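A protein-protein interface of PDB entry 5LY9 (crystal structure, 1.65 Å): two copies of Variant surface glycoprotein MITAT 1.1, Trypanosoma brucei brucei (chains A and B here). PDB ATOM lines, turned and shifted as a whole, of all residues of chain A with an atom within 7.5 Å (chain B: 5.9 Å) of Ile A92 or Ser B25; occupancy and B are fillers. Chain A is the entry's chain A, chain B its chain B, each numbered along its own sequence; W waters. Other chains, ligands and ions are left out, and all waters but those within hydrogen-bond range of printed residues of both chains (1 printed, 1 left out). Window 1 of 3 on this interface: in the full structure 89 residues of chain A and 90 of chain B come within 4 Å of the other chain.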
ATOM      1  N   SER A  25     -17.129 -13.405  22.590  1.00  0.00           N
ATOM      2  CA  SER A  25     -17.551 -12.617  21.418  1.00  0.00           C
ATOM      3  C   SER A  25     -18.037 -11.267  21.827  1.00  0.00           C
ATOM      4  O   SER A  25     -17.642 -10.212  21.262  1.00  0.00           O
ATOM      5  CB  SER A  25     -18.571 -13.345  20.560  1.00  0.00           C
ATOM      6  OG  SER A  25     -17.939 -14.554  20.125  1.00  0.00           O
ATOM      7  N   MET A  28     -15.285  -9.140  23.049  1.00  0.00           N
ATOM      8  CA  MET A  28     -14.646  -8.568  21.918  1.00  0.00           C
ATOM      9  C   MET A  28     -15.448  -7.386  21.284  1.00  0.00           C
ATOM     10  O   MET A  28     -14.852  -6.359  20.837  1.00  0.00           O
ATOM     11  CB  MET A  28     -14.245  -9.646  20.921  1.00  0.00           C
ATOM     12  CG  MET A  28     -13.160 -10.568  21.428  1.00  0.00           C
ATOM     13  SD  MET A  28     -11.624  -9.662  21.771  1.00  0.00           S
ATOM     14  CE  MET A  28     -11.746  -9.146  23.483  1.00  0.00           C
ATOM     15  N   TYR A  83      -5.979   0.081  14.359  1.00  0.00           N
ATOM     16  CA  TYR A  83      -7.133  -0.797  14.549  1.00  0.00           C
ATOM     17  C   TYR A  83      -7.443  -1.585  13.226  1.00  0.00           C
ATOM     18  O   TYR A  83      -7.661  -2.782  13.227  1.00  0.00           O
ATOM     19  CB  TYR A  83      -8.380  -0.022  15.022  1.00  0.00           C
ATOM     20  CG  TYR A  83      -9.489  -0.962  15.485  1.00  0.00           C
ATOM     21  CD1 TYR A  83      -9.273  -1.865  16.469  1.00  0.00           C
ATOM     22  CD2 TYR A  83     -10.704  -0.921  14.926  1.00  0.00           C
ATOM     23  CE1 TYR A  83     -10.291  -2.719  16.911  1.00  0.00           C
ATOM     24  CE2 TYR A  83     -11.722  -1.775  15.333  1.00  0.00           C
ATOM     25  CZ  TYR A  83     -11.502  -2.637  16.344  1.00  0.00           C
ATOM     26  OH  TYR A  83     -12.511  -3.494  16.745  1.00  0.00           O
ATOM     27  N   GLY A  87      -5.384  -4.351  15.064  1.00  0.00           N
ATOM     28  CA  GLY A  87      -6.243  -4.529  16.229  1.00  0.00           C
ATOM     29  C   GLY A  87      -7.513  -5.336  16.004  1.00  0.00           C
ATOM     30  O   GLY A  87      -7.887  -6.239  16.798  1.00  0.00           O
ATOM     31  N   LEU A  88      -8.211  -5.016  14.930  1.00  0.00           N
ATOM     32  CA  LEU A  88      -9.487  -5.661  14.670  1.00  0.00           C
ATOM     33  C   LEU A  88      -9.298  -7.144  14.450  1.00  0.00           C
ATOM     34  O   LEU A  88     -10.117  -7.939  14.929  1.00  0.00           O
ATOM     35  CB  LEU A  88     -10.153  -5.041  13.475  1.00  0.00           C
ATOM     36  CG  LEU A  88     -11.410  -5.689  12.883  1.00  0.00           C
ATOM     37  CD1 LEU A  88     -12.533  -5.630  13.869  1.00  0.00           C
ATOM     38  CD2 LEU A  88     -11.796  -5.022  11.614  1.00  0.00           C
ATOM     39  N   ALA A  89      -8.243  -7.523  13.762  1.00  0.00           N
ATOM     40  CA  ALA A  89      -7.948  -8.913  13.518  1.00  0.00           C
ATOM     41  C   ALA A  89      -7.845  -9.657  14.823  1.00  0.00           C
ATOM     42  O   ALA A  89      -8.297 -10.817  14.944  1.00  0.00           O
ATOM     43  CB  ALA A  89      -6.673  -9.091  12.696  1.00  0.00           C
ATOM     44  N   THR A  90      -7.202  -9.048  15.812  1.00  0.00           N
ATOM     45  CA  THR A  90      -6.989  -9.777  17.088  1.00  0.00           C
ATOM     46  C   THR A  90      -8.332 -10.099  17.768  1.00  0.00           C
ATOM     47  O   THR A  90      -8.444 -11.114  18.470  1.00  0.00           O
ATOM     48  CB  THR A  90      -6.108  -9.007  18.114  1.00  0.00           C
ATOM     49  OG1 THR A  90      -6.844  -7.844  18.608  1.00  0.00           O
ATOM     50  CG2 THR A  90      -4.760  -8.606  17.506  1.00  0.00           C
ATOM     51  N   GLN A  91      -9.279  -9.208  17.565  1.00  0.00           N
ATOM     52  CA  GLN A  91     -10.586  -9.294  18.265  1.00  0.00           C
ATOM     53  C   GLN A  91     -11.501 -10.293  17.564  1.00  0.00           C
ATOM     54  O   GLN A  91     -12.084 -11.169  18.210  1.00  0.00           O
ATOM     55  CB  GLN A  91     -11.185  -7.945  18.458  1.00  0.00           C
ATOM     56  CG  GLN A  91     -10.356  -7.028  19.341  1.00  0.00           C
ATOM     57  CD  GLN A  91     -10.866  -5.620  19.478  1.00  0.00           C
ATOM     58  OE1 GLN A  91     -11.749  -5.176  18.760  1.00  0.00           O
ATOM     59  NE2 GLN A  91     -10.345  -4.929  20.470  1.00  0.00           N
ATOM     60  N   ILE A  92     -11.511 -10.243  16.226  1.00  0.00           N
ATOM     61  CA  ILE A  92     -12.185 -11.270  15.433  1.00  0.00           C
ATOM     62  C   ILE A  92     -11.540 -12.649  15.673  1.00  0.00           C
ATOM     63  O   ILE A  92     -12.264 -13.688  15.835  1.00  0.00           O
ATOM     64  CB  ILE A  92     -12.221 -10.895  13.951  1.00  0.00           C
ATOM     65  CG1 ILE A  92     -13.141  -9.670  13.777  1.00  0.00           C
ATOM     66  CG2 ILE A  92     -12.756 -12.038  13.103  1.00  0.00           C
ATOM     67  CD1 ILE A  92     -13.111  -9.210  12.338  1.00  0.00           C
ATOM     68  N   ARG A  93     -10.228 -12.686  15.679  1.00  0.00           N
ATOM     69  CA  ARG A  93      -9.511 -13.934  15.884  1.00  0.00           C
ATOM     70  C   ARG A  93      -9.960 -14.570  17.222  1.00  0.00           C
ATOM     71  O   ARG A  93     -10.273 -15.781  17.315  1.00  0.00           O
ATOM     72  CB  ARG A  93      -8.012 -13.735  15.895  1.00  0.00           C
ATOM     73  CG  ARG A  93      -7.219 -14.985  16.062  1.00  0.00           C
ATOM     74  CD  ARG A  93      -5.811 -14.695  16.499  1.00  0.00           C
ATOM     75  NE  ARG A  93      -5.076 -15.939  16.673  1.00  0.00           N
ATOM     76  CZ  ARG A  93      -3.851 -15.983  17.143  1.00  0.00           C
ATOM     77  NH1 ARG A  93      -3.183 -14.853  17.455  1.00  0.00           N
ATOM     78  NH2 ARG A  93      -3.248 -17.134  17.233  1.00  0.00           N
ATOM     79  N   SER A  94      -9.990 -13.775  18.292  1.00  0.00           N
ATOM     80  CA  SER A  94     -10.332 -14.332  19.594  1.00  0.00           C
ATOM     81  C   SER A  94     -11.806 -14.739  19.678  1.00  0.00           C
ATOM     82  O   SER A  94     -12.136 -15.822  20.216  1.00  0.00           O
ATOM     83  CB  SER A  94     -10.018 -13.340  20.729  1.00  0.00           C
ATOM     84  OG  SER A  94     -10.256 -13.902  22.013  1.00  0.00           O
ATOM     85  N   ALA A  95     -12.686 -13.903  19.184  1.00  0.00           N
ATOM     86  CA  ALA A  95     -14.124 -14.259  19.139  1.00  0.00           C
ATOM     87  C   ALA A  95     -14.309 -15.584  18.402  1.00  0.00           C
ATOM     88  O   ALA A  95     -14.987 -16.467  18.926  1.00  0.00           O
ATOM     89  CB  ALA A  95     -14.949 -13.142  18.534  1.00  0.00           C
ATOM     90  N   ARG A  96     -13.685 -15.777  17.254  1.00  0.00           N
ATOM     91  CA  ARG A  96     -13.937 -16.996  16.462  1.00  0.00           C
ATOM     92  C   ARG A  96     -13.203 -18.179  17.054  1.00  0.00           C
ATOM     93  O   ARG A  96     -13.683 -19.326  16.931  1.00  0.00           O
ATOM     94  CB  ARG A  96     -13.622 -16.780  14.995  1.00  0.00           C
ATOM     95  CG  ARG A  96     -12.165 -16.684  14.604  1.00  0.00           C
ATOM     96  CD  ARG A  96     -11.704 -18.061  14.193  1.00  0.00           C
ATOM     97  NE  ARG A  96     -10.357 -18.170  13.567  1.00  0.00           N
ATOM     98  CZ  ARG A  96      -9.221 -18.199  14.237  1.00  0.00           C
ATOM     99  NH1 ARG A  96      -9.145 -17.910  15.546  1.00  0.00           N
ATOM    100  NH2 ARG A  96      -8.100 -18.436  13.596  1.00  0.00           N
ATOM    101  N   ALA A  97     -12.084 -17.939  17.718  1.00  0.00           N
ATOM    102  CA  ALA A  97     -11.315 -19.050  18.295  1.00  0.00           C
ATOM    103  C   ALA A  97     -12.128 -19.616  19.451  1.00  0.00           C
ATOM    104  O   ALA A  97     -12.302 -20.868  19.589  1.00  0.00           O
ATOM    105  CB  ALA A  97     -10.011 -18.568  18.801  1.00  0.00           C
ATOM    106  N   ALA A  98     -12.631 -18.714  20.272  1.00  0.00           N
ATOM    107  CA  ALA A  98     -13.464 -19.159  21.416  1.00  0.00           C
ATOM    108  C   ALA A  98     -14.728 -19.872  20.937  1.00  0.00           C
ATOM    109  O   ALA A  98     -15.069 -20.946  21.479  1.00  0.00           O
ATOM    110  CB  ALA A  98     -13.853 -17.968  22.307  1.00  0.00           C
ATOM    111  N   GLU A 248      -5.232 -22.316  19.905  1.00  0.00           N
ATOM    112  CA  GLU A 248      -5.663 -21.145  19.231  1.00  0.00           C
ATOM    113  C   GLU A 248      -6.540 -20.230  20.098  1.00  0.00           C
ATOM    114  O   GLU A 248      -6.315 -19.021  20.152  1.00  0.00           O
ATOM    115  CB  GLU A 248      -6.394 -21.504  17.927  1.00  0.00           C
ATOM    116  CG  GLU A 248      -6.991 -20.293  17.238  1.00  0.00           C
ATOM    117  CD  GLU A 248      -5.986 -19.287  16.670  1.00  0.00           C
ATOM    118  OE1 GLU A 248      -4.768 -19.509  16.662  1.00  0.00           O
ATOM    119  OE2 GLU A 248      -6.446 -18.242  16.204  1.00  0.00           O
ATOM    120  N   ALA A 252      -5.057 -16.630  21.105  1.00  0.00           N
ATOM    121  CA  ALA A 252      -5.824 -15.499  20.634  1.00  0.00           C
ATOM    122  C   ALA A 252      -6.324 -14.675  21.815  1.00  0.00           C
ATOM    123  O   ALA A 252      -6.373 -13.453  21.754  1.00  0.00           O
ATOM    124  CB  ALA A 252      -6.995 -15.971  19.808  1.00  0.00           C
ATOM    125  N   LEU B  21     -17.500 -22.321   5.738  1.00  0.00           N
ATOM    126  CA  LEU B  21     -17.522 -21.595   7.013  1.00  0.00           C
ATOM    127  C   LEU B  21     -16.146 -21.249   7.492  1.00  0.00           C
ATOM    128  O   LEU B  21     -15.962 -20.229   8.173  1.00  0.00           O
ATOM    129  CB  LEU B  21     -18.276 -22.372   8.098  1.00  0.00           C
ATOM    130  CG  LEU B  21     -19.765 -22.660   7.858  1.00  0.00           C
ATOM    131  CD1 LEU B  21     -20.328 -23.602   8.917  1.00  0.00           C
ATOM    132  CD2 LEU B  21     -20.618 -21.388   7.727  1.00  0.00           C
ATOM    133  N   SER B  22     -15.143 -21.980   7.043  1.00  0.00           N
ATOM    134  CA  SER B  22     -13.768 -21.749   7.500  1.00  0.00           C
ATOM    135  C   SER B  22     -13.248 -20.333   7.166  1.00  0.00           C
ATOM    136  O   SER B  22     -12.402 -19.825   7.844  1.00  0.00           O
ATOM    137  CB  SER B  22     -12.838 -22.849   6.921  1.00  0.00           C
ATOM    138  OG  SER B  22     -12.547 -22.582   5.559  1.00  0.00           O
ATOM    139  N   LYS B  23     -13.762 -19.737   6.095  1.00  0.00           N
ATOM    140  CA  LYS B  23     -13.353 -18.403   5.670  1.00  0.00           C
ATOM    141  C   LYS B  23     -14.198 -17.297   6.116  1.00  0.00           C
ATOM    142  O   LYS B  23     -13.843 -16.115   5.848  1.00  0.00           O
ATOM    143  CB  LYS B  23     -13.166 -18.301   4.135  1.00  0.00           C
ATOM    144  CG  LYS B  23     -12.110 -19.301   3.600  1.00  0.00           C
ATOM    145  CD  LYS B  23     -11.707 -18.946   2.178  1.00  0.00           C
ATOM    146  CE  LYS B  23     -10.603 -19.861   1.667  1.00  0.00           C
ATOM    147  NZ  LYS B  23     -10.231 -19.364   0.309  1.00  0.00           N
ATOM    148  N   VAL B  24     -15.282 -17.561   6.842  1.00  0.00           N
ATOM    149  CA  VAL B  24     -16.215 -16.494   7.164  1.00  0.00           C
ATOM    150  C   VAL B  24     -15.494 -15.453   8.078  1.00  0.00           C
ATOM    151  O   VAL B  24     -15.717 -14.265   7.933  1.00  0.00           O
ATOM    152  CB  VAL B  24     -17.487 -17.034   7.803  1.00  0.00           C
ATOM    153  CG1 VAL B  24     -18.298 -15.904   8.376  1.00  0.00           C
ATOM    154  CG2 VAL B  24     -18.319 -17.750   6.787  1.00  0.00           C
ATOM    155  N   SER B  25     -14.719 -15.919   9.062  1.00  0.00           N
ATOM    156  CA  SER B  25     -14.013 -15.003   9.935  1.00  0.00           C
ATOM    157  C   SER B  25     -13.097 -14.061   9.197  1.00  0.00           C
ATOM    158  O   SER B  25     -13.090 -12.836   9.455  1.00  0.00           O
ATOM    159  CB  SER B  25     -13.238 -15.748  11.033  1.00  0.00           C
ATOM    160  OG  SER B  25     -14.215 -16.425  11.894  1.00  0.00           O
ATOM    161  N   GLY B  26     -12.338 -14.609   8.254  1.00  0.00           N
ATOM    162  CA  GLY B  26     -11.441 -13.803   7.438  1.00  0.00           C
ATOM    163  C   GLY B  26     -12.167 -12.848   6.535  1.00  0.00           C
ATOM    164  O   GLY B  26     -11.726 -11.718   6.302  1.00  0.00           O
ATOM    165  N   GLU B  27     -13.300 -13.254   6.017  1.00  0.00           N
ATOM    166  CA  GLU B  27     -14.118 -12.335   5.262  1.00  0.00           C
ATOM    167  C   GLU B  27     -14.671 -11.192   6.157  1.00  0.00           C
ATOM    168  O   GLU B  27     -14.751 -10.075   5.709  1.00  0.00           O
ATOM    169  CB  GLU B  27     -15.203 -13.037   4.485  1.00  0.00           C
ATOM    170  CG  GLU B  27     -16.129 -12.037   3.799  1.00  0.00           C
ATOM    171  CD  GLU B  27     -17.042 -12.588   2.695  1.00  0.00           C
ATOM    172  OE1 GLU B  27     -16.566 -13.375   1.815  1.00  0.00           O
ATOM    173  OE2 GLU B  27     -18.182 -12.023   2.595  1.00  0.00           O
ATOM    174  N   MET B  28     -15.041 -11.459   7.395  1.00  0.00           N
ATOM    175  CA  MET B  28     -15.496 -10.422   8.290  1.00  0.00           C
ATOM    176  C   MET B  28     -14.360  -9.467   8.649  1.00  0.00           C
ATOM    177  O   MET B  28     -14.604  -8.274   8.699  1.00  0.00           O
ATOM    178  CB  MET B  28     -16.178 -11.019   9.510  1.00  0.00           C
ATOM    179  CG  MET B  28     -17.514 -11.661   9.209  1.00  0.00           C
ATOM    180  SD  MET B  28     -18.676 -10.436   8.619  1.00  0.00           S
ATOM    181  CE  MET B  28     -18.575 -10.579   6.870  1.00  0.00           C
ATOM    182  N   LEU B  29     -13.140  -9.971   8.782  1.00  0.00           N
ATOM    183  CA  LEU B  29     -11.933  -9.129   8.956  1.00  0.00           C
ATOM    184  C   LEU B  29     -11.774  -8.216   7.726  1.00  0.00           C
ATOM    185  O   LEU B  29     -11.657  -6.979   7.870  1.00  0.00           O
ATOM    186  CB  LEU B  29     -10.657  -9.951   9.180  1.00  0.00           C
ATOM    187  CG  LEU B  29      -9.360  -9.158   9.215  1.00  0.00           C
ATOM    188  CD1 LEU B  29      -9.410  -8.001  10.249  1.00  0.00           C
ATOM    189  CD2 LEU B  29      -8.119 -10.014   9.397  1.00  0.00           C
ATOM    190  N   ASN B  30     -11.818  -8.812   6.548  1.00  0.00           N
ATOM    191  CA  ASN B  30     -11.754  -7.996   5.314  1.00  0.00           C
ATOM    192  C   ASN B  30     -12.840  -6.925   5.249  1.00  0.00           C
ATOM    193  O   ASN B  30     -12.576  -5.758   4.868  1.00  0.00           O
ATOM    194  CB  ASN B  30     -11.785  -8.866   4.059  1.00  0.00           C
ATOM    195  CG  ASN B  30     -11.551  -8.055   2.822  1.00  0.00           C
ATOM    196  OD1 ASN B  30     -10.497  -7.518   2.682  1.00  0.00           O
ATOM    197  ND2 ASN B  30     -12.583  -7.893   1.972  1.00  0.00           N
ATOM    198  N   LEU B  88     -19.903  -3.133  13.720  1.00  0.00           N
ATOM    199  CA  LEU B  88     -18.938  -4.019  14.230  1.00  0.00           C
ATOM    200  C   LEU B  88     -19.618  -5.228  14.873  1.00  0.00           C
ATOM    201  O   LEU B  88     -19.225  -6.340  14.646  1.00  0.00           O
ATOM    202  CB  LEU B  88     -18.073  -3.363  15.318  1.00  0.00           C
ATOM    203  CG  LEU B  88     -17.081  -4.227  16.049  1.00  0.00           C
ATOM    204  CD1 LEU B  88     -16.101  -4.909  15.089  1.00  0.00           C
ATOM    205  CD2 LEU B  88     -16.323  -3.444  17.124  1.00  0.00           C
ATOM    206  N   GLN B  91     -20.494  -8.016  12.399  1.00  0.00           N
ATOM    207  CA  GLN B  91     -19.384  -8.732  11.826  1.00  0.00           C
ATOM    208  C   GLN B  91     -18.816  -9.736  12.823  1.00  0.00           C
ATOM    209  O   GLN B  91     -18.495 -10.881  12.461  1.00  0.00           O
ATOM    210  CB  GLN B  91     -18.326  -7.750  11.324  1.00  0.00           C
ATOM    211  CG  GLN B  91     -18.892  -6.883  10.159  1.00  0.00           C
ATOM    212  CD  GLN B  91     -17.938  -5.858   9.665  1.00  0.00           C
ATOM    213  OE1 GLN B  91     -16.916  -5.558  10.285  1.00  0.00           O
ATOM    214  NE2 GLN B  91     -18.240  -5.317   8.533  1.00  0.00           N
ATOM    215  N   ILE B  92     -18.672  -9.341  14.097  1.00  0.00           N
ATOM    216  CA  ILE B  92     -18.290 -10.281  15.166  1.00  0.00           C
ATOM    217  C   ILE B  92     -19.394 -11.400  15.328  1.00  0.00           C
ATOM    218  O   ILE B  92     -19.114 -12.589  15.408  1.00  0.00           O
ATOM    219  CB  ILE B  92     -18.108  -9.559  16.492  1.00  0.00           C
ATOM    220  CG1 ILE B  92     -16.805  -8.749  16.402  1.00  0.00           C
ATOM    221  CG2 ILE B  92     -17.935 -10.563  17.657  1.00  0.00           C
ATOM    222  CD1 ILE B  92     -16.612  -7.792  17.562  1.00  0.00           C
ATOM    223  N   ALA B  95     -18.969 -13.793  12.327  1.00  0.00           N
ATOM    224  CA  ALA B  95     -17.741 -14.622  12.514  1.00  0.00           C
ATOM    225  C   ALA B  95     -17.973 -15.723  13.562  1.00  0.00           C
ATOM    226  O   ALA B  95     -17.610 -16.872  13.360  1.00  0.00           O
ATOM    227  CB  ALA B  95     -16.567 -13.760  12.950  1.00  0.00           C
ATOM    228  N   ARG B  96     -18.484 -15.332  14.713  1.00  0.00           N
ATOM    229  CA  ARG B  96     -18.607 -16.286  15.825  1.00  0.00           C
ATOM    230  C   ARG B  96     -19.709 -17.289  15.577  1.00  0.00           C
ATOM    231  O   ARG B  96     -19.623 -18.448  16.024  1.00  0.00           O
ATOM    232  CB  ARG B  96     -18.681 -15.658  17.189  1.00  0.00           C
ATOM    233  CG  ARG B  96     -20.003 -14.976  17.484  1.00  0.00           C
ATOM    234  CD  ARG B  96     -20.953 -15.982  18.194  1.00  0.00           C
ATOM    235  NE  ARG B  96     -22.183 -15.400  18.716  1.00  0.00           N
ATOM    236  CZ  ARG B  96     -23.322 -15.177  18.034  1.00  0.00           C
ATOM    237  NH1 ARG B  96     -23.399 -15.336  16.727  1.00  0.00           N
ATOM    238  NH2 ARG B  96     -24.442 -14.874  18.666  1.00  0.00           N
ATOM    239  N   ALA B  98     -20.610 -18.512  12.573  1.00  0.00           N
ATOM    240  CA  ALA B  98     -20.057 -19.468  11.682  1.00  0.00           C
ATOM    241  C   ALA B  98     -19.086 -20.387  12.361  1.00  0.00           C
ATOM    242  O   ALA B  98     -19.085 -21.608  12.103  1.00  0.00           O
ATOM    243  CB  ALA B  98     -19.365 -18.747  10.548  1.00  0.00           C
ATOM    244  N   ALA B  99     -18.223 -19.785  13.192  1.00  0.00           N
ATOM    245  CA  ALA B  99     -17.232 -20.574  13.932  1.00  0.00           C
ATOM    246  C   ALA B  99     -17.850 -21.581  14.927  1.00  0.00           C
ATOM    247  O   ALA B  99     -17.385 -22.698  15.015  1.00  0.00           O
ATOM    248  CB  ALA B  99     -16.239 -19.627  14.642  1.00  0.00           C
ATOM    249  N   MET B 149      -9.606 -24.905  11.696  1.00  0.00           N
ATOM    250  CA  MET B 149      -9.893 -23.516  11.428  1.00  0.00           C
ATOM    251  C   MET B 149      -8.587 -22.858  10.982  1.00  0.00           C
ATOM    252  O   MET B 149      -7.602 -22.897  11.698  1.00  0.00           O
ATOM    253  CB  MET B 149     -10.498 -22.861  12.707  1.00  0.00           C
ATOM    254  CG  MET B 149     -10.793 -21.355  12.593  1.00  0.00           C
ATOM    255  SD  MET B 149     -12.250 -21.055  11.544  1.00  0.00           S
ATOM    256  CE  MET B 149     -13.592 -21.411  12.705  1.00  0.00           C
ATOM    257  N   THR B 152      -6.847 -16.265  10.823  1.00  0.00           N
ATOM    258  CA  THR B 152      -7.738 -15.238  10.495  1.00  0.00           C
ATOM    259  C   THR B 152      -6.974 -14.184   9.709  1.00  0.00           C
ATOM    260  O   THR B 152      -6.089 -13.547  10.237  1.00  0.00           O
ATOM    261  CB  THR B 152      -8.343 -14.558  11.742  1.00  0.00           C
ATOM    262  OG1 THR B 152      -9.076 -15.529  12.498  1.00  0.00           O
ATOM    263  CG2 THR B 152      -9.298 -13.435  11.317  1.00  0.00           C
ATOM    264  N   LYS B 153      -7.312 -14.095   8.444  1.00  0.00           N
ATOM    265  CA  LYS B 153      -6.668 -13.162   7.537  1.00  0.00           C
ATOM    266  C   LYS B 153      -7.710 -12.727   6.475  1.00  0.00           C
ATOM    267  O   LYS B 153      -8.699 -13.392   6.279  1.00  0.00           O
ATOM    268  CB  LYS B 153      -5.473 -13.804   6.950  1.00  0.00           C
ATOM    269  CG  LYS B 153      -5.771 -14.903   5.965  1.00  0.00           C
ATOM    270  CD  LYS B 153      -4.488 -15.682   5.728  1.00  0.00           C
ATOM    271  CE  LYS B 153      -4.653 -16.656   4.544  1.00  0.00           C
ATOM    272  NZ  LYS B 153      -4.469 -15.860   3.270  1.00  0.00           N
HETATM  273  O   HOH W   1     -10.027 -17.784  10.683  1.00  0.00           O
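OG1 of Thr B152 lies within hydrogen-bond range of NE of Arg A96.
The backbone NH (N) of Leu A88 sits at hydrogen-bond distance from the backbone carbonyl oxygen (O) of Tyr A83, 2.9 Å away. OH of Tyr A83 lies within hydrogen-bond range of OE1 of Gln A91 (2.7 Å). NH1 of Arg A96 sits at hydrogen-bond distance from O of Arg A93, at 3.0 Å. NE of Arg A93 lies within salt-bridge range of OE2 of Glu A248 (2.7 Å). The guanidinium group (NH1) of Arg A96 is in salt-bridge range of the side-chain carboxylate (OE2) of Glu A248 (2.8 Å).
Among the printed residues, merely in contact across the chains: Ser A25 with Ile B92 (3.6 Å), Ser A25 with Arg B96 (3.2 Å), Met A28 with Ile B92 (3.9 Å), Tyr A83 with Leu B88 (3.8 Å), Leu A88 with Leu B88 (3.8 Å), Ala A89 with Leu B29 (3.7 Å), Ile A92 with Ser B25 (3.7 Å), Ile A92 with Met B28 (3.9 Å), Ile A92 with Leu B29 (3.6 Å), Arg A93 with Thr B152 (3.8 Å), Arg A96 with Ser B25 (3.2 Å), Arg A96 with Ala B99 (3.4 Å) and Arg A96 with Met B149 (3.4 Å).
Printed residues of chain B within 4 Å of Tyr A83: Leu B88 (3.8 Å). Ile A92 touches just these residues of chain B: Ser B25, Met B28 and Leu B29. Ala A252 touches none of the printed residues of chain B. Ser B25 touches just these residues of chain A: Ile A92 (3.7 Å) and Arg A96 (3.2 Å). Of the printed residues of chain A, Leu B29 touches Ala A89 and Ile A92. The nearest residue of chain B that does not touch Ile A92 is Thr B152 (4.1 Å).
Hydrophobic or aromatic side chains of chain B that line the printed part of chain A: Leu B29, Leu B88, Ile B92, Ala B99 and Met B149. Hydrophobic or aromatic side chains of chain A that line the printed part of chain B: Tyr A83, Leu A88, Ala A89 and Ile A92. Among the printed residues, 14 pairs touch across the chains.
Ser A25 touches Ile B92, and with the chains exchanged Ile A92 touches Ser B25. Ser A25 touches Arg B96, and with the chains exchanged Arg A96 touches Ser B25. Met A28 touches Ile B92, and with the chains exchanged Ile A92 touches Met B28. Leu A88 touches its own counterpart, Leu B88. 8 positions are printed for both chains. Of the 14 pairs that touch across the chains among the printed residues, 7 have their exchanged pair printed and touching as well.
Water W1 bridges the guanidinium group (NE) of Arg A96 (2.9 Å) and the side-chain hydroxyl (OG1) of Thr B152 (3.0 Å).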
